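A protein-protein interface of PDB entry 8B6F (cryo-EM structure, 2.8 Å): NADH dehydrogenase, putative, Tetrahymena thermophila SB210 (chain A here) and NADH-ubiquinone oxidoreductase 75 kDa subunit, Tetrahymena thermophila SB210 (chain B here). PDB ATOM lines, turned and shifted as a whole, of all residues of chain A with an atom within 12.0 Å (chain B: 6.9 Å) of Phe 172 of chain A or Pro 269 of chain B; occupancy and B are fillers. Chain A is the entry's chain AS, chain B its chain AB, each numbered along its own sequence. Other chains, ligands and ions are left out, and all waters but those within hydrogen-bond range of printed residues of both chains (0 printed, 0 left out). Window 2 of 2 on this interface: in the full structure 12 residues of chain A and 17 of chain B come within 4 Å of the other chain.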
ATOM      1  N   GLY A 166     -29.094   0.374  30.939  1.00  0.00           N
ATOM      2  CA  GLY A 166     -28.590   0.405  29.583  1.00  0.00           C
ATOM      3  C   GLY A 166     -27.874   1.706  29.259  1.00  0.00           C
ATOM      4  O   GLY A 166     -28.008   2.716  29.946  1.00  0.00           O
ATOM      5  N   ASN A 167     -27.091   1.665  28.177  1.00  0.00           N
ATOM      6  CA  ASN A 167     -26.329   2.835  27.757  1.00  0.00           C
ATOM      7  C   ASN A 167     -26.382   3.045  26.246  1.00  0.00           C
ATOM      8  O   ASN A 167     -25.496   3.707  25.692  1.00  0.00           O
ATOM      9  CB  ASN A 167     -24.869   2.721  28.204  1.00  0.00           C
ATOM     10  CG  ASN A 167     -24.148   1.568  27.542  1.00  0.00           C
ATOM     11  OD1 ASN A 167     -24.754   0.553  27.205  1.00  0.00           O
ATOM     12  ND2 ASN A 167     -22.844   1.720  27.350  1.00  0.00           N
ATOM     13  N   LYS A 168     -27.392   2.497  25.565  1.00  0.00           N
ATOM     14  CA  LYS A 168     -27.502   2.628  24.121  1.00  0.00           C
ATOM     15  C   LYS A 168     -28.946   2.376  23.729  1.00  0.00           C
ATOM     16  O   LYS A 168     -29.587   1.507  24.336  1.00  0.00           O
ATOM     17  CB  LYS A 168     -26.581   1.631  23.408  1.00  0.00           C
ATOM     18  CG  LYS A 168     -26.508   1.816  21.902  1.00  0.00           C
ATOM     19  CD  LYS A 168     -25.917   0.595  21.215  1.00  0.00           C
ATOM     20  CE  LYS A 168     -26.944  -0.515  21.070  1.00  0.00           C
ATOM     21  NZ  LYS A 168     -28.057  -0.134  20.153  1.00  0.00           N
ATOM     22  N   PRO A 169     -29.494   3.094  22.749  1.00  0.00           N
ATOM     23  CA  PRO A 169     -30.847   2.768  22.284  1.00  0.00           C
ATOM     24  C   PRO A 169     -30.919   1.332  21.790  1.00  0.00           C
ATOM     25  O   PRO A 169     -30.022   0.846  21.098  1.00  0.00           O
ATOM     26  CB  PRO A 169     -31.086   3.770  21.150  1.00  0.00           C
ATOM     27  CG  PRO A 169     -30.174   4.902  21.443  1.00  0.00           C
ATOM     28  CD  PRO A 169     -28.961   4.296  22.084  1.00  0.00           C
ATOM     29  N   THR A 170     -32.003   0.649  22.154  1.00  0.00           N
ATOM     30  CA  THR A 170     -32.180  -0.749  21.789  1.00  0.00           C
ATOM     31  C   THR A 170     -32.882  -0.938  20.451  1.00  0.00           C
ATOM     32  O   THR A 170     -32.843  -2.044  19.902  1.00  0.00           O
ATOM     33  CB  THR A 170     -32.972  -1.483  22.877  1.00  0.00           C
ATOM     34  OG1 THR A 170     -34.229  -0.827  23.086  1.00  0.00           O
ATOM     35  CG2 THR A 170     -32.191  -1.502  24.180  1.00  0.00           C
ATOM     36  N   GLU A 171     -33.516   0.107  19.914  1.00  0.00           N
ATOM     37  CA  GLU A 171     -34.191  -0.028  18.627  1.00  0.00           C
ATOM     38  C   GLU A 171     -33.198  -0.318  17.510  1.00  0.00           C
ATOM     39  O   GLU A 171     -33.468  -1.143  16.629  1.00  0.00           O
ATOM     40  CB  GLU A 171     -34.985   1.239  18.314  1.00  0.00           C
ATOM     41  CG  GLU A 171     -36.268   1.381  19.108  1.00  0.00           C
ATOM     42  CD  GLU A 171     -37.299   0.329  18.746  1.00  0.00           C
ATOM     43  OE1 GLU A 171     -37.117  -0.354  17.717  1.00  0.00           O
ATOM     44  OE2 GLU A 171     -38.292   0.183  19.489  1.00  0.00           O
ATOM     45  N   PHE A 172     -32.051   0.352  17.523  1.00  0.00           N
ATOM     46  CA  PHE A 172     -31.032   0.147  16.502  1.00  0.00           C
ATOM     47  C   PHE A 172     -29.773  -0.455  17.117  1.00  0.00           C
ATOM     48  O   PHE A 172     -28.905   0.266  17.607  1.00  0.00           O
ATOM     49  CB  PHE A 172     -30.699   1.465  15.801  1.00  0.00           C
ATOM     50  CG  PHE A 172     -29.838   1.298  14.585  1.00  0.00           C
ATOM     51  CD1 PHE A 172     -28.460   1.243  14.699  1.00  0.00           C
ATOM     52  CD2 PHE A 172     -30.408   1.194  13.328  1.00  0.00           C
ATOM     53  CE1 PHE A 172     -27.666   1.090  13.582  1.00  0.00           C
ATOM     54  CE2 PHE A 172     -29.619   1.042  12.208  1.00  0.00           C
ATOM     55  CZ  PHE A 172     -28.246   0.988  12.335  1.00  0.00           C
ATOM     56  N   THR B 266     -15.108   1.451   9.048  1.00  0.00           N
ATOM     57  CA  THR B 266     -16.526   1.611   9.321  1.00  0.00           C
ATOM     58  C   THR B 266     -16.985   3.006   8.927  1.00  0.00           C
ATOM     59  O   THR B 266     -16.269   3.989   9.140  1.00  0.00           O
ATOM     60  CB  THR B 266     -16.842   1.374  10.798  1.00  0.00           C
ATOM     61  OG1 THR B 266     -16.304   2.444  11.584  1.00  0.00           O
ATOM     62  CG2 THR B 266     -16.235   0.068  11.261  1.00  0.00           C
ATOM     63  N   ARG B 267     -18.180   3.082   8.356  1.00  0.00           N
ATOM     64  CA  ARG B 267     -18.872   4.341   8.102  1.00  0.00           C
ATOM     65  C   ARG B 267     -20.081   4.359   9.033  1.00  0.00           C
ATOM     66  O   ARG B 267     -21.176   3.939   8.661  1.00  0.00           O
ATOM     67  CB  ARG B 267     -19.285   4.470   6.640  1.00  0.00           C
ATOM     68  CG  ARG B 267     -19.997   5.775   6.326  1.00  0.00           C
ATOM     69  CD  ARG B 267     -20.635   5.750   4.951  1.00  0.00           C
ATOM     70  NE  ARG B 267     -21.374   6.979   4.688  1.00  0.00           N
ATOM     71  CZ  ARG B 267     -22.115   7.194   3.611  1.00  0.00           C
ATOM     72  NH1 ARG B 267     -22.245   6.277   2.666  1.00  0.00           N
ATOM     73  NH2 ARG B 267     -22.744   8.358   3.479  1.00  0.00           N
ATOM     74  N   GLY B 268     -19.874   4.854  10.249  1.00  0.00           N
ATOM     75  CA  GLY B 268     -20.899   4.811  11.262  1.00  0.00           C
ATOM     76  C   GLY B 268     -21.073   3.407  11.803  1.00  0.00           C
ATOM     77  O   GLY B 268     -20.101   2.667  11.978  1.00  0.00           O
ATOM     78  N   PRO B 269     -22.316   3.006  12.082  1.00  0.00           N
ATOM     79  CA  PRO B 269     -22.531   1.649  12.610  1.00  0.00           C
ATOM     80  C   PRO B 269     -22.043   0.549  11.685  1.00  0.00           C
ATOM     81  O   PRO B 269     -21.619  -0.508  12.167  1.00  0.00           O
ATOM     82  CB  PRO B 269     -24.055   1.587  12.799  1.00  0.00           C
ATOM     83  CG  PRO B 269     -24.492   2.999  12.896  1.00  0.00           C
ATOM     84  CD  PRO B 269     -23.569   3.775  12.015  1.00  0.00           C
ATOM     85  N   GLU B 270     -22.082   0.764  10.373  1.00  0.00           N
ATOM     86  CA  GLU B 270     -21.805  -0.298   9.417  1.00  0.00           C
ATOM     87  C   GLU B 270     -20.309  -0.550   9.282  1.00  0.00           C
ATOM     88  O   GLU B 270     -19.509   0.387   9.216  1.00  0.00           O
ATOM     89  CB  GLU B 270     -22.399   0.058   8.055  1.00  0.00           C
ATOM     90  CG  GLU B 270     -23.879   0.397   8.112  1.00  0.00           C
ATOM     91  CD  GLU B 270     -24.465   0.693   6.750  1.00  0.00           C
ATOM     92  OE1 GLU B 270     -23.802   0.388   5.738  1.00  0.00           O
ATOM     93  OE2 GLU B 270     -25.589   1.234   6.690  1.00  0.00           O
ATOM     94  N   ILE B 271     -19.939  -1.831   9.231  1.00  0.00           N
ATOM     95  CA  ILE B 271     -18.556  -2.259   9.058  1.00  0.00           C
ATOM     96  C   ILE B 271     -18.367  -2.714   7.620  1.00  0.00           C
ATOM     97  O   ILE B 271     -19.285  -3.246   6.986  1.00  0.00           O
ATOM     98  CB  ILE B 271     -18.187  -3.386  10.050  1.00  0.00           C
ATOM     99  CG1 ILE B 271     -18.332  -2.898  11.495  1.00  0.00           C
ATOM    100  CG2 ILE B 271     -16.772  -3.882   9.789  1.00  0.00           C
ATOM    101  CD1 ILE B 271     -18.174  -3.988  12.534  1.00  0.00           C
ATOM    102  N   VAL B 603     -14.976  -1.681  18.042  1.00  0.00           N
ATOM    103  CA  VAL B 603     -15.232  -0.917  16.829  1.00  0.00           C
ATOM    104  C   VAL B 603     -16.629  -0.313  16.843  1.00  0.00           C
ATOM    105  O   VAL B 603     -16.794   0.891  16.648  1.00  0.00           O
ATOM    106  CB  VAL B 603     -15.017  -1.814  15.590  1.00  0.00           C
ATOM    107  CG1 VAL B 603     -15.326  -1.054  14.318  1.00  0.00           C
ATOM    108  CG2 VAL B 603     -13.594  -2.348  15.562  1.00  0.00           C
ATOM    109  N   VAL B 604     -17.650  -1.138  17.072  1.00  0.00           N
ATOM    110  CA  VAL B 604     -19.023  -0.677  17.230  1.00  0.00           C
ATOM    111  C   VAL B 604     -19.634  -1.395  18.425  1.00  0.00           C
ATOM    112  O   VAL B 604     -19.243  -2.514  18.765  1.00  0.00           O
ATOM    113  CB  VAL B 604     -19.871  -0.912  15.960  1.00  0.00           C
ATOM    114  CG1 VAL B 604     -19.358  -0.061  14.814  1.00  0.00           C
ATOM    115  CG2 VAL B 604     -19.865  -2.382  15.576  1.00  0.00           C
ATOM    116  N   PRO B 606     -22.388  -3.389  20.815  1.00  0.00           N
ATOM    117  CA  PRO B 606     -23.191  -4.576  20.505  1.00  0.00           C
ATOM    118  C   PRO B 606     -24.558  -4.188  19.972  1.00  0.00           C
ATOM    119  O   PRO B 606     -25.140  -3.184  20.406  1.00  0.00           O
ATOM    120  CB  PRO B 606     -23.302  -5.292  21.861  1.00  0.00           C
ATOM    121  CG  PRO B 606     -22.149  -4.800  22.646  1.00  0.00           C
ATOM    122  CD  PRO B 606     -21.943  -3.382  22.218  1.00  0.00           C
ATOM    123  N   PRO B 607     -25.105  -4.954  19.030  1.00  0.00           N
ATOM    124  CA  PRO B 607     -26.385  -4.572  18.427  1.00  0.00           C
ATOM    125  C   PRO B 607     -27.540  -4.677  19.409  1.00  0.00           C
ATOM    126  O   PRO B 607     -27.561  -5.533  20.297  1.00  0.00           O
ATOM    127  CB  PRO B 607     -26.545  -5.575  17.280  1.00  0.00           C
ATOM    128  CG  PRO B 607     -25.808  -6.769  17.738  1.00  0.00           C
ATOM    129  CD  PRO B 607     -24.633  -6.255  18.526  1.00  0.00           C
ATOM    130  N   GLY B 608     -28.514  -3.792  19.231  1.00  0.00           N
ATOM    131  CA  GLY B 608     -29.728  -3.868  20.025  1.00  0.00           C
ATOM    132  C   GLY B 608     -29.441  -3.772  21.508  1.00  0.00           C
ATOM    133  O   GLY B 608     -28.718  -2.885  21.973  1.00  0.00           O
ATOM    134  N   ASP B 609     -30.017  -4.702  22.270  1.00  0.00           N
ATOM    135  CA  ASP B 609     -29.909  -4.714  23.721  1.00  0.00           C
ATOM    136  C   ASP B 609     -28.807  -5.646  24.212  1.00  0.00           C
ATOM    137  O   ASP B 609     -28.780  -5.995  25.396  1.00  0.00           O
ATOM    138  CB  ASP B 609     -31.248  -5.113  24.340  1.00  0.00           C
ATOM    139  CG  ASP B 609     -31.410  -4.608  25.760  1.00  0.00           C
ATOM    140  OD1 ASP B 609     -30.386  -4.301  26.406  1.00  0.00           O
ATOM    141  OD2 ASP B 609     -32.562  -4.516  26.231  1.00  0.00           O
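The backbone carbonyl oxygen (O) of Gly 608 of chain B lies close to the side-chain amino group (NZ) of Lys 168 of chain A, 3.4 Å away.
Hydrophobic or aromatic side chains of chain B within 4 Å of the printed part of chain A: Pro 269.
Along chain B the printed residues that touch a printed residue of chain A span positions 269 to 609.
Of the 7 printed residues of chain A, 3 touch a printed residue of chain B.
Printed residues of chain A that touch a printed residue of chain B: Lys 168, Thr 170 and Phe 172.
Among the printed residues, no Asp or Glu carboxylate lies within 4 Å of a Lys or Arg side-chain nitrogen of the other chain.
Of the printed residues of chain B, Thr 170 of chain A touches Gly 608 (3.6 Å) and Asp 609 (3.6 Å).
Glu 171 of chain A touches none of the printed residues of chain B.
Of the printed residues of chain B, Phe 172 of chain A touches Pro 269.
No residue of chain A comes within 4 Å of Thr 266 of chain B.
Arg 267 of chain B touches none of the printed residues of chain A.
Gly 268 of chain B touches none of the printed residues of chain A.
Of chain A, only Phe 172 comes within 4 Å of Pro 269 of chain B.
No residue of chain A comes within 4 Å of Ile 271 of chain B.
Of the printed residues of chain A, Pro 606 of chain B touches Lys 168.
No residue of chain A comes within 4 Å of Pro 607 of chain B.
Gly 608 of chain B touches just these residues of chain A: Lys 168 (3.1 Å) and Thr 170 (3.6 Å).
The nearest residue of chain B that does not touch Phe 172 of chain A is Gly 608 of chain B (4.1 Å).
The nearest residue of chain A that does not touch Pro 269 of chain B is Lys 168 of chain A (8.5 Å).
The nearest printed residue of chain B that does not touch Lys 168 of chain A is Pro 607 of chain B (4.5 Å).
O of Phe 172 of chain A sits at hydrogen-bond distance from NZ of Lys 168 of chain A.
Among the printed residues, pairs that only touch across the chains: Lys 168 of chain A with Pro 606 of chain B, Thr 170 of chain A with Gly 608 of chain B, Thr 170 of chain A with Asp 609 of chain B and Phe 172 of chain A with Pro 269 of chain B.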
